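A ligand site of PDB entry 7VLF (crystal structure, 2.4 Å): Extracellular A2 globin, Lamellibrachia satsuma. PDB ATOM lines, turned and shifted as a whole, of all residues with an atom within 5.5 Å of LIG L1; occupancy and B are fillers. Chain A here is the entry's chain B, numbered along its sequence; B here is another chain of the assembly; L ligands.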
ATOM      1  N   ALA A  43      -8.898  26.883  23.907  1.00  0.00           N
ATOM      2  CA  ALA A  43      -8.771  25.468  24.237  1.00  0.00           C
ATOM      3  C   ALA A  43      -8.880  25.206  25.737  1.00  0.00           C
ATOM      4  O   ALA A  43      -9.240  24.093  26.131  1.00  0.00           O
ATOM      5  CB  ALA A  43      -7.453  24.919  23.701  1.00  0.00           C
ATOM      6  N   MET A  46     -12.007  23.413  27.022  1.00  0.00           N
ATOM      7  CA  MET A  46     -12.205  21.977  26.914  1.00  0.00           C
ATOM      8  C   MET A  46     -11.702  21.213  28.132  1.00  0.00           C
ATOM      9  O   MET A  46     -12.102  20.066  28.335  1.00  0.00           O
ATOM     10  CB  MET A  46     -11.511  21.458  25.656  1.00  0.00           C
ATOM     11  CG  MET A  46     -11.760  22.301  24.418  1.00  0.00           C
ATOM     12  SD  MET A  46     -11.237  21.423  22.942  1.00  0.00           S
ATOM     13  CE  MET A  46     -12.152  19.898  23.164  1.00  0.00           C
ATOM     14  N   PHE A  47     -10.831  21.826  28.924  1.00  0.00           N
ATOM     15  CA  PHE A  47     -10.239  21.148  30.072  1.00  0.00           C
ATOM     16  C   PHE A  47     -10.722  21.770  31.373  1.00  0.00           C
ATOM     17  O   PHE A  47      -9.916  22.128  32.233  1.00  0.00           O
ATOM     18  CB  PHE A  47      -8.716  21.184  29.989  1.00  0.00           C
ATOM     19  CG  PHE A  47      -8.171  20.677  28.679  1.00  0.00           C
ATOM     20  CD1 PHE A  47      -7.855  19.344  28.508  1.00  0.00           C
ATOM     21  CD2 PHE A  47      -7.956  21.550  27.629  1.00  0.00           C
ATOM     22  CE1 PHE A  47      -7.350  18.881  27.306  1.00  0.00           C
ATOM     23  CE2 PHE A  47      -7.456  21.100  26.423  1.00  0.00           C
ATOM     24  CZ  PHE A  47      -7.148  19.758  26.260  1.00  0.00           C
ATOM     25  N   LYS A  48     -12.045  21.894  31.529  1.00  0.00           N
ATOM     26  CA  LYS A  48     -12.596  22.480  32.740  1.00  0.00           C
ATOM     27  C   LYS A  48     -12.405  21.563  33.948  1.00  0.00           C
ATOM     28  O   LYS A  48     -12.186  22.031  35.071  1.00  0.00           O
ATOM     29  CB  LYS A  48     -14.084  22.778  32.537  1.00  0.00           C
ATOM     30  CG  LYS A  48     -14.747  23.458  33.725  1.00  0.00           C
ATOM     31  CD  LYS A  48     -16.214  23.772  33.439  1.00  0.00           C
ATOM     32  CE  LYS A  48     -16.868  24.427  34.637  1.00  0.00           C
ATOM     33  NZ  LYS A  48     -18.299  24.739  34.371  1.00  0.00           N
ATOM     34  N   ARG A  49     -12.490  20.248  33.731  1.00  0.00           N
ATOM     35  CA  ARG A  49     -12.474  19.301  34.845  1.00  0.00           C
ATOM     36  C   ARG A  49     -11.118  19.230  35.525  1.00  0.00           C
ATOM     37  O   ARG A  49     -11.046  19.037  36.743  1.00  0.00           O
ATOM     38  CB  ARG A  49     -12.902  17.914  34.365  1.00  0.00           C
ATOM     39  CG  ARG A  49     -13.352  16.986  35.477  1.00  0.00           C
ATOM     40  CD  ARG A  49     -13.913  15.692  34.928  1.00  0.00           C
ATOM     41  NE  ARG A  49     -12.873  14.706  34.628  1.00  0.00           N
ATOM     42  CZ  ARG A  49     -12.445  13.786  35.481  1.00  0.00           C
ATOM     43  NH1 ARG A  49     -12.970  13.724  36.697  1.00  0.00           N
ATOM     44  NH2 ARG A  49     -11.497  12.930  35.129  1.00  0.00           N
ATOM     45  N   VAL A  50     -10.035  19.388  34.761  1.00  0.00           N
ATOM     46  CA  VAL A  50      -8.685  19.269  35.306  1.00  0.00           C
ATOM     47  C   VAL A  50      -8.201  20.636  35.764  1.00  0.00           C
ATOM     48  O   VAL A  50      -7.021  20.820  36.053  1.00  0.00           O
ATOM     49  CB  VAL A  50      -7.720  18.668  34.276  1.00  0.00           C
ATOM     50  CG1 VAL A  50      -8.228  17.310  33.803  1.00  0.00           C
ATOM     51  CG2 VAL A  50      -7.545  19.612  33.097  1.00  0.00           C
ATOM     52  N   HIS A  63      -3.189  15.879  34.754  1.00  0.00           N
ATOM     53  CA  HIS A  63      -3.671  15.735  33.376  1.00  0.00           C
ATOM     54  C   HIS A  63      -2.512  15.818  32.389  1.00  0.00           C
ATOM     55  O   HIS A  63      -2.455  15.044  31.433  1.00  0.00           O
ATOM     56  CB  HIS A  63      -4.714  16.801  33.066  1.00  0.00           C
ATOM     57  CG  HIS A  63      -5.078  16.871  31.610  1.00  0.00           C
ATOM     58  ND1 HIS A  63      -5.953  15.989  31.017  1.00  0.00           N
ATOM     59  CD2 HIS A  63      -4.670  17.715  30.629  1.00  0.00           C
ATOM     60  CE1 HIS A  63      -6.068  16.285  29.733  1.00  0.00           C
ATOM     61  NE2 HIS A  63      -5.299  17.332  29.478  1.00  0.00           N
ATOM     62  N   ARG A  66      -1.033  12.667  32.326  1.00  0.00           N
ATOM     63  CA  ARG A  66      -1.828  11.696  31.573  1.00  0.00           C
ATOM     64  C   ARG A  66      -1.525  11.782  30.075  1.00  0.00           C
ATOM     65  O   ARG A  66      -1.248  10.761  29.429  1.00  0.00           O
ATOM     66  CB  ARG A  66      -3.323  11.933  31.832  1.00  0.00           C
ATOM     67  CG  ARG A  66      -4.003  10.821  32.591  1.00  0.00           C
ATOM     68  CD  ARG A  66      -4.600  11.325  33.884  1.00  0.00           C
ATOM     69  NE  ARG A  66      -5.453  12.490  33.686  1.00  0.00           N
ATOM     70  CZ  ARG A  66      -5.875  13.290  34.664  1.00  0.00           C
ATOM     71  NH1 ARG A  66      -6.640  14.328  34.389  1.00  0.00           N
ATOM     72  NH2 ARG A  66      -5.508  13.052  35.918  1.00  0.00           N
ATOM     73  N   VAL A  67      -1.562  12.989  29.520  1.00  0.00           N
ATOM     74  CA  VAL A  67      -1.379  13.149  28.080  1.00  0.00           C
ATOM     75  C   VAL A  67       0.075  12.877  27.688  1.00  0.00           C
ATOM     76  O   VAL A  67       0.339  12.307  26.625  1.00  0.00           O
ATOM     77  CB  VAL A  67      -1.848  14.542  27.629  1.00  0.00           C
ATOM     78  CG1 VAL A  67      -1.553  14.757  26.162  1.00  0.00           C
ATOM     79  CG2 VAL A  67      -3.326  14.729  27.930  1.00  0.00           C
ATOM     80  N   GLY A  70       0.432   9.074  27.827  1.00  0.00           N
ATOM     81  CA  GLY A  70      -0.245   8.485  26.686  1.00  0.00           C
ATOM     82  C   GLY A  70       0.509   8.711  25.385  1.00  0.00           C
ATOM     83  O   GLY A  70       0.582   7.811  24.542  1.00  0.00           O
ATOM     84  N   LEU A  71       1.080   9.902  25.213  1.00  0.00           N
ATOM     85  CA  LEU A  71       1.891  10.179  24.028  1.00  0.00           C
ATOM     86  C   LEU A  71       3.173   9.364  24.033  1.00  0.00           C
ATOM     87  O   LEU A  71       3.651   8.961  22.969  1.00  0.00           O
ATOM     88  CB  LEU A  71       2.187  11.670  23.937  1.00  0.00           C
ATOM     89  CG  LEU A  71       3.053  12.140  22.760  1.00  0.00           C
ATOM     90  CD1 LEU A  71       2.495  11.618  21.454  1.00  0.00           C
ATOM     91  CD2 LEU A  71       3.157  13.666  22.739  1.00  0.00           C
ATOM     92  N   CYS A  74       2.554   5.894  22.367  1.00  0.00           N
ATOM     93  CA  CYS A  74       2.472   5.863  20.917  1.00  0.00           C
ATOM     94  C   CYS A  74       3.857   6.004  20.293  1.00  0.00           C
ATOM     95  O   CYS A  74       4.172   5.328  19.302  1.00  0.00           O
ATOM     96  CB  CYS A  74       1.547   6.964  20.423  1.00  0.00           C
ATOM     97  SG  CYS A  74      -0.070   6.956  21.216  1.00  0.00           S
ATOM     98  N   LEU A  91      -7.143   5.462  22.134  1.00  0.00           N
ATOM     99  CA  LEU A  91      -7.216   6.897  22.413  1.00  0.00           C
ATOM    100  C   LEU A  91      -8.250   7.590  21.535  1.00  0.00           C
ATOM    101  O   LEU A  91      -8.771   8.641  21.921  1.00  0.00           O
ATOM    102  CB  LEU A  91      -5.838   7.531  22.208  1.00  0.00           C
ATOM    103  CG  LEU A  91      -4.750   7.134  23.214  1.00  0.00           C
ATOM    104  CD1 LEU A  91      -3.417   7.746  22.813  1.00  0.00           C
ATOM    105  CD2 LEU A  91      -5.140   7.550  24.618  1.00  0.00           C
ATOM    106  N   GLN A  94     -11.814   7.667  23.325  1.00  0.00           N
ATOM    107  CA  GLN A  94     -11.994   8.621  24.424  1.00  0.00           C
ATOM    108  C   GLN A  94     -12.051  10.057  23.920  1.00  0.00           C
ATOM    109  O   GLN A  94     -12.749  10.892  24.512  1.00  0.00           O
ATOM    110  CB  GLN A  94     -10.861   8.453  25.437  1.00  0.00           C
ATOM    111  CG  GLN A  94     -10.610   7.012  25.831  1.00  0.00           C
ATOM    112  CD  GLN A  94      -9.304   6.841  26.570  1.00  0.00           C
ATOM    113  OE1 GLN A  94      -8.551   7.798  26.755  1.00  0.00           O
ATOM    114  NE2 GLN A  94      -9.019   5.621  27.002  1.00  0.00           N
ATOM    115  N   HIS A  95     -11.326  10.374  22.853  1.00  0.00           N
ATOM    116  CA  HIS A  95     -11.252  11.741  22.355  1.00  0.00           C
ATOM    117  C   HIS A  95     -12.355  12.100  21.370  1.00  0.00           C
ATOM    118  O   HIS A  95     -12.525  13.286  21.069  1.00  0.00           O
ATOM    119  CB  HIS A  95      -9.888  11.987  21.689  1.00  0.00           C
ATOM    120  CG  HIS A  95      -8.785  12.267  22.662  1.00  0.00           C
ATOM    121  ND1 HIS A  95      -8.207  11.284  23.438  1.00  0.00           N
ATOM    122  CD2 HIS A  95      -8.165  13.428  23.001  1.00  0.00           C
ATOM    123  CE1 HIS A  95      -7.271  11.821  24.199  1.00  0.00           C
ATOM    124  NE2 HIS A  95      -7.231  13.121  23.950  1.00  0.00           N
ATOM    125  N   ARG A  98     -15.120  14.207  23.164  1.00  0.00           N
ATOM    126  CA  ARG A  98     -14.819  15.613  23.406  1.00  0.00           C
ATOM    127  C   ARG A  98     -15.120  16.485  22.189  1.00  0.00           C
ATOM    128  O   ARG A  98     -15.242  17.707  22.341  1.00  0.00           O
ATOM    129  CB  ARG A  98     -13.350  15.775  23.793  1.00  0.00           C
ATOM    130  CG  ARG A  98     -12.650  14.500  24.226  1.00  0.00           C
ATOM    131  CD  ARG A  98     -12.941  14.135  25.676  1.00  0.00           C
ATOM    132  NE  ARG A  98     -12.170  12.963  26.096  1.00  0.00           N
ATOM    133  CZ  ARG A  98     -12.194  12.454  27.316  1.00  0.00           C
ATOM    134  NH1 ARG A  98     -11.461  11.384  27.602  1.00  0.00           N
ATOM    135  NH2 ARG A  98     -12.948  13.002  28.255  1.00  0.00           N
ATOM    136  N   VAL A 100     -13.096  17.121  19.684  1.00  0.00           N
ATOM    137  CA  VAL A 100     -11.913  17.962  19.517  1.00  0.00           C
ATOM    138  C   VAL A 100     -11.757  18.345  18.056  1.00  0.00           C
ATOM    139  O   VAL A 100     -11.893  17.512  17.152  1.00  0.00           O
ATOM    140  CB  VAL A 100     -10.670  17.245  20.053  1.00  0.00           C
ATOM    141  CG1 VAL A 100     -10.719  17.141  21.570  1.00  0.00           C
ATOM    142  CG2 VAL A 100     -10.580  15.854  19.460  1.00  0.00           C
ATOM    143  N   GLN A 104      -7.039  21.673  16.548  1.00  0.00           N
ATOM    144  CA  GLN A 104      -6.557  21.604  17.918  1.00  0.00           C
ATOM    145  C   GLN A 104      -5.462  20.556  18.080  1.00  0.00           C
ATOM    146  O   GLN A 104      -4.554  20.728  18.904  1.00  0.00           O
ATOM    147  CB  GLN A 104      -7.719  21.321  18.870  1.00  0.00           C
ATOM    148  CG  GLN A 104      -8.717  22.457  18.980  1.00  0.00           C
ATOM    149  CD  GLN A 104      -9.925  22.087  19.816  1.00  0.00           C
ATOM    150  OE1 GLN A 104     -10.499  21.011  19.650  1.00  0.00           O
ATOM    151  NE2 GLN A 104     -10.295  22.975  20.725  1.00  0.00           N
ATOM    152  N   TYR A 105      -5.524  19.469  17.300  1.00  0.00           N
ATOM    153  CA  TYR A 105      -4.422  18.507  17.287  1.00  0.00           C
ATOM    154  C   TYR A 105      -3.152  19.146  16.728  1.00  0.00           C
ATOM    155  O   TYR A 105      -2.056  18.917  17.254  1.00  0.00           O
ATOM    156  CB  TYR A 105      -4.799  17.269  16.482  1.00  0.00           C
ATOM    157  CG  TYR A 105      -5.692  16.298  17.211  1.00  0.00           C
ATOM    158  CD1 TYR A 105      -5.168  15.447  18.188  1.00  0.00           C
ATOM    159  CD2 TYR A 105      -7.039  16.207  16.927  1.00  0.00           C
ATOM    160  CE1 TYR A 105      -5.980  14.555  18.856  1.00  0.00           C
ATOM    161  CE2 TYR A 105      -7.850  15.315  17.594  1.00  0.00           C
ATOM    162  CZ  TYR A 105      -7.319  14.493  18.559  1.00  0.00           C
ATOM    163  OH  TYR A 105      -8.131  13.601  19.226  1.00  0.00           O
ATOM    164  N   VAL A 108      -1.403  21.298  19.452  1.00  0.00           N
ATOM    165  CA  VAL A 108      -0.616  20.523  20.414  1.00  0.00           C
ATOM    166  C   VAL A 108       0.499  19.774  19.706  1.00  0.00           C
ATOM    167  O   VAL A 108       1.553  19.507  20.296  1.00  0.00           O
ATOM    168  CB  VAL A 108      -1.520  19.576  21.213  1.00  0.00           C
ATOM    169  CG1 VAL A 108      -2.781  20.287  21.659  1.00  0.00           C
ATOM    170  CG2 VAL A 108      -1.847  18.319  20.417  1.00  0.00           C
ATOM    171  N   ILE A 137       0.324   9.992  14.608  1.00  0.00           N
ATOM    172  CA  ILE A 137      -0.266   9.759  15.922  1.00  0.00           C
ATOM    173  C   ILE A 137      -1.632  10.432  16.024  1.00  0.00           C
ATOM    174  O   ILE A 137      -2.615   9.820  16.461  1.00  0.00           O
ATOM    175  CB  ILE A 137       0.676  10.243  17.034  1.00  0.00           C
ATOM    176  CG1 ILE A 137       2.058   9.598  16.867  1.00  0.00           C
ATOM    177  CG2 ILE A 137       0.105   9.917  18.400  1.00  0.00           C
ATOM    178  CD1 ILE A 137       3.061  10.050  17.903  1.00  0.00           C
ATOM    179  N   THR A 138      -1.709  11.704  15.608  1.00  0.00           N
ATOM    180  CA  THR A 138      -2.975  12.415  15.690  1.00  0.00           C
ATOM    181  C   THR A 138      -4.013  11.856  14.724  1.00  0.00           C
ATOM    182  O   THR A 138      -5.210  11.857  15.021  1.00  0.00           O
ATOM    183  CB  THR A 138      -2.768  13.910  15.431  1.00  0.00           C
ATOM    184  OG1 THR A 138      -2.080  14.085  14.183  1.00  0.00           O
ATOM    185  CG2 THR A 138      -1.952  14.535  16.550  1.00  0.00           C
ATOM    186  N   ILE A 141      -5.891   8.989  16.285  1.00  0.00           N
ATOM    187  CA  ILE A 141      -6.839   9.403  17.313  1.00  0.00           C
ATOM    188  C   ILE A 141      -8.069  10.044  16.694  1.00  0.00           C
ATOM    189  O   ILE A 141      -9.163  10.011  17.277  1.00  0.00           O
ATOM    190  CB  ILE A 141      -6.153  10.354  18.322  1.00  0.00           C
ATOM    191  CG1 ILE A 141      -4.815   9.774  18.770  1.00  0.00           C
ATOM    192  CG2 ILE A 141      -7.040  10.593  19.522  1.00  0.00           C
ATOM    193  CD1 ILE A 141      -4.029  10.680  19.693  1.00  0.00           C
ATOM    194  N   HIS B  94      -7.274   9.779  40.752  1.00  0.00           N
ATOM    195  CA  HIS B  94      -7.877   9.528  39.441  1.00  0.00           C
ATOM    196  C   HIS B  94      -7.929   8.033  39.147  1.00  0.00           C
ATOM    197  O   HIS B  94      -8.978   7.496  38.776  1.00  0.00           O
ATOM    198  CB  HIS B  94      -7.091  10.270  38.355  1.00  0.00           C
ATOM    199  CG  HIS B  94      -7.589  10.015  36.976  1.00  0.00           C
ATOM    200  ND1 HIS B  94      -8.456  10.876  36.326  1.00  0.00           N
ATOM    201  CD2 HIS B  94      -7.345   9.011  36.098  1.00  0.00           C
ATOM    202  CE1 HIS B  94      -8.722  10.405  35.118  1.00  0.00           C
ATOM    203  NE2 HIS B  94      -8.065   9.277  34.964  1.00  0.00           N
ATOM    204  N   GLN B  98     -11.030   5.457  38.993  1.00  0.00           N
ATOM    205  CA  GLN B  98     -11.128   4.811  37.692  1.00  0.00           C
ATOM    206  C   GLN B  98     -11.273   3.297  37.804  1.00  0.00           C
ATOM    207  O   GLN B  98     -11.913   2.687  36.945  1.00  0.00           O
ATOM    208  CB  GLN B  98      -9.901   5.153  36.848  1.00  0.00           C
ATOM    209  CG  GLN B  98      -9.907   4.593  35.433  1.00  0.00           C
ATOM    210  CD  GLN B  98      -8.571   4.765  34.729  1.00  0.00           C
ATOM    211  OE1 GLN B  98      -7.545   4.276  35.192  1.00  0.00           O
ATOM    212  NE2 GLN B  98      -8.581   5.476  33.604  1.00  0.00           N
HETATM  213  C1  LIG L   1      -7.915  13.661  28.169  1.00  0.00           C
HETATM  214  C2  LIG L   1      -4.029  12.131  25.779  1.00  0.00           C
HETATM  215  C3  LIG L   1      -4.980  15.282  22.263  1.00  0.00           C
HETATM  216  C4  LIG L   1      -8.656  17.053  24.741  1.00  0.00           C
HETATM  217  C5  LIG L   1      -6.826  12.936  27.791  1.00  0.00           C
HETATM  218  C6  LIG L   1      -6.311  11.744  28.464  1.00  0.00           C
HETATM  219  C7  LIG L   1      -5.244  11.331  27.796  1.00  0.00           C
HETATM  220  C8  LIG L   1      -5.048  12.233  26.694  1.00  0.00           C
HETATM  221  C9  LIG L   1      -4.385  10.108  28.146  1.00  0.00           C
HETATM  222  C10 LIG L   1      -6.873  11.035  29.706  1.00  0.00           C
HETATM  223  C11 LIG L   1      -8.270  10.473  29.398  1.00  0.00           C
HETATM  224  C12 LIG L   1      -8.864   9.787  30.606  1.00  0.00           C
HETATM  225  O1  LIG L   1     -10.112   9.779  30.724  1.00  0.00           O
HETATM  226  O2  LIG L   1      -8.091   9.253  31.459  1.00  0.00           O
HETATM  227  C13 LIG L   1      -4.016  12.814  24.601  1.00  0.00           C
HETATM  228  C14 LIG L   1      -3.141  12.523  23.487  1.00  0.00           C
HETATM  229  C15 LIG L   1      -3.417  13.413  22.515  1.00  0.00           C
HETATM  230  C16 LIG L   1      -4.470  14.261  23.007  1.00  0.00           C
HETATM  231  C17 LIG L   1      -2.089  11.388  23.488  1.00  0.00           C
HETATM  232  C18 LIG L   1      -2.817  13.623  21.094  1.00  0.00           C
HETATM  233  C19 LIG L   1      -1.576  14.052  20.825  1.00  0.00           C
HETATM  234  C20 LIG L   1      -5.974  16.089  22.680  1.00  0.00           C
HETATM  235  C21 LIG L   1      -6.308  17.342  22.052  1.00  0.00           C
HETATM  236  C22 LIG L   1      -7.350  17.841  22.731  1.00  0.00           C
HETATM  237  C23 LIG L   1      -7.653  16.915  23.811  1.00  0.00           C
HETATM  238  C24 LIG L   1      -5.593  17.910  20.818  1.00  0.00           C
HETATM  239  C25 LIG L   1      -8.085  19.177  22.488  1.00  0.00           C
HETATM  240  C26 LIG L   1      -7.482  20.227  21.930  1.00  0.00           C
HETATM  241  C27 LIG L   1      -8.824  16.268  25.848  1.00  0.00           C
HETATM  242  C28 LIG L   1      -9.905  16.425  26.777  1.00  0.00           C
HETATM  243  C29 LIG L   1      -9.663  15.344  27.846  1.00  0.00           C
HETATM  244  C30 LIG L   1      -8.463  14.685  27.449  1.00  0.00           C
HETATM  245  C31 LIG L   1     -11.057  17.439  26.705  1.00  0.00           C
HETATM  246  C32 LIG L   1     -10.481  15.046  29.089  1.00  0.00           C
HETATM  247  C33 LIG L   1     -10.351  16.276  29.964  1.00  0.00           C
HETATM  248  C34 LIG L   1     -10.759  15.922  31.369  1.00  0.00           C
HETATM  249  O3  LIG L   1     -10.477  14.757  31.800  1.00  0.00           O
HETATM  250  O4  LIG L   1     -11.359  16.805  32.032  1.00  0.00           O
HETATM  251  N1  LIG L   1      -6.009  13.229  26.723  1.00  0.00           N
HETATM  252  N2  LIG L   1      -4.829  13.881  24.282  1.00  0.00           N
HETATM  253  N3  LIG L   1      -6.788  15.858  23.762  1.00  0.00           N
HETATM  254  N4  LIG L   1      -7.993  15.234  26.277  1.00  0.00           N
HETATM  255 FE1  LIG L   1      -6.427  14.584  25.329  1.00  0.00          FE
HETATM  256  C1  LG2 L   2      -7.116  -0.646  33.444  1.00  0.00           C
HETATM  257  C2  LG2 L   2      -3.149   1.003  35.693  1.00  0.00           C
HETATM  258  C3  LG2 L   2      -3.331  -2.780  38.737  1.00  0.00           C
HETATM  259  C4  LG2 L   2      -7.703  -3.975  37.002  1.00  0.00           C
HETATM  260  C5  LG2 L   2      -5.985   0.087  33.745  1.00  0.00           C
HETATM  261  C6  LG2 L   2      -5.442   1.185  32.957  1.00  0.00           C
HETATM  262  C7  LG2 L   2      -4.349   1.636  33.578  1.00  0.00           C
HETATM  263  C8  LG2 L   2      -4.159   0.848  34.785  1.00  0.00           C
HETATM  264  C9  LG2 L   2      -3.425   2.791  33.125  1.00  0.00           C
HETATM  265  C10 LG2 L   2      -6.054   1.704  31.628  1.00  0.00           C
HETATM  266  C11 LG2 L   2      -6.625   3.109  31.793  1.00  0.00           C
HETATM  267  C12 LG2 L   2      -7.247   3.556  30.495  1.00  0.00           C
HETATM  268  O1  LG2 L   2      -7.306   4.785  30.261  1.00  0.00           O
HETATM  269  O2  LG2 L   2      -7.671   2.676  29.704  1.00  0.00           O
HETATM  270  C13 LG2 L   2      -2.821   0.105  36.696  1.00  0.00           C
HETATM  271  C14 LG2 L   2      -1.648   0.139  37.532  1.00  0.00           C
HETATM  272  C15 LG2 L   2      -1.699  -0.894  38.367  1.00  0.00           C
HETATM  273  C16 LG2 L   2      -2.913  -1.639  38.092  1.00  0.00           C
HETATM  274  C17 LG2 L   2      -0.519   1.200  37.481  1.00  0.00           C
HETATM  275  C18 LG2 L   2      -0.640  -1.249  39.443  1.00  0.00           C
HETATM  276  C19 LG2 L   2      -0.759  -0.779  40.687  1.00  0.00           C
HETATM  277  C20 LG2 L   2      -4.525  -3.428  38.548  1.00  0.00           C
HETATM  278  C21 LG2 L   2      -4.981  -4.600  39.271  1.00  0.00           C
HETATM  279  C22 LG2 L   2      -6.180  -4.942  38.803  1.00  0.00           C
HETATM  280  C23 LG2 L   2      -6.549  -3.996  37.756  1.00  0.00           C
HETATM  281  C24 LG2 L   2      -4.209  -5.331  40.380  1.00  0.00           C
HETATM  282  C25 LG2 L   2      -6.986  -6.152  39.333  1.00  0.00           C
HETATM  283  C26 LG2 L   2      -8.133  -6.564  38.779  1.00  0.00           C
HETATM  284  C27 LG2 L   2      -7.930  -3.249  35.855  1.00  0.00           C
HETATM  285  C28 LG2 L   2      -9.040  -3.443  34.944  1.00  0.00           C
HETATM  286  C29 LG2 L   2      -8.844  -2.402  33.829  1.00  0.00           C
HETATM  287  C30 LG2 L   2      -7.651  -1.682  34.179  1.00  0.00           C
HETATM  288  C31 LG2 L   2     -10.176  -4.481  35.057  1.00  0.00           C
HETATM  289  C32 LG2 L   2      -9.747  -2.163  32.595  1.00  0.00           C
HETATM  290  C33 LG2 L   2      -9.226  -2.993  31.424  1.00  0.00           C
HETATM  291  C34 LG2 L   2      -9.910  -2.567  30.153  1.00  0.00           C
HETATM  292  O3  LG2 L   2     -10.322  -3.463  29.371  1.00  0.00           O
HETATM  293  O4  LG2 L   2     -10.057  -1.338  29.939  1.00  0.00           O
HETATM  294  N1  LG2 L   2      -5.176  -0.084  34.854  1.00  0.00           N
HETATM  295  N2  LG2 L   2      -3.578  -0.991  37.059  1.00  0.00           N
HETATM  296  N3  LG2 L   2      -5.510  -3.093  37.635  1.00  0.00           N
HETATM  297  N4  LG2 L   2      -7.147  -2.202  35.364  1.00  0.00           N
HETATM  298 FE1  LG2 L   2      -5.393  -1.592  36.252  1.00  0.00          FE
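O of Met 46 touches C31 of LIG L1, at 3.3 Å.
CE1 of Phe 47 touches C27 of LIG L1 (3.3 Å).
Val 50 touches LIG L1 (CG1 to O4, 3.6 Å).
CE1 of His 63 touches C1 of LIG L1, at 3.6 Å.
O of Arg 66 touches C9 of LIG L1, 3.5 Å away.
Val 67 touches LIG L1.
N of Leu 71 touches C17 of LIG L1 (3.9 Å).
Leu 91 touches LIG L1 (CD1 to C17, 3.9 Å).
Gln 94 of chain A touches LIG L1.
Val 100 touches LIG L1 (CG1 to C25, 3.5 Å).
CB of Gln 104 touches C26 of LIG L1, at 3.3 Å.
Tyr 105 touches LIG L1 (CE1 to C3, 3.6 Å).
CG1 of Val 108 touches C24 of LIG L1 (3.8 Å).
CD1 of Ile 141 touches C18 of LIG L1, 3.5 Å away.
His 94 of chain B touches LIG L1 (NE2 to O2, 3.5 Å).
Hydrophobic or aromatic side chains within 4 Å of LIG L1: Met 46, Phe 47, Val 50, His 63, Val 67, Leu 91, His 95, Val 100, Tyr 105, Val 108, Ile 141 and His 94 of chain B.
The nearest printed residue that does not touch LIG L1 is Gly 70 (4.2 Å).
NE2 of His 95 binds FE1 of LIG L1 (2.2 Å).
O4 of LIG L1 lies within salt-bridge range of NE of Arg 49, 3.7 Å away.
The guanidinium group (NH1) of Arg 98 of chain A lies within salt-bridge range of an oxygen (O1) of LIG L1, at 3.8 Å.
A ring nitrogen (ND1) of His 95 is in hydrogen-bond range of the backbone carbonyl oxygen of Leu 91, 3.1 Å away.
The side-chain amide nitrogen of Gln 104 sits at hydrogen-bond distance from the side-chain sulfur of Met 46 (2.9 Å).
The guanidinium group (NE) of Arg 98 of chain A lies within hydrogen-bond range of the backbone carbonyl oxygen (O) of Gln 94 of chain A, 2.7 Å away.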
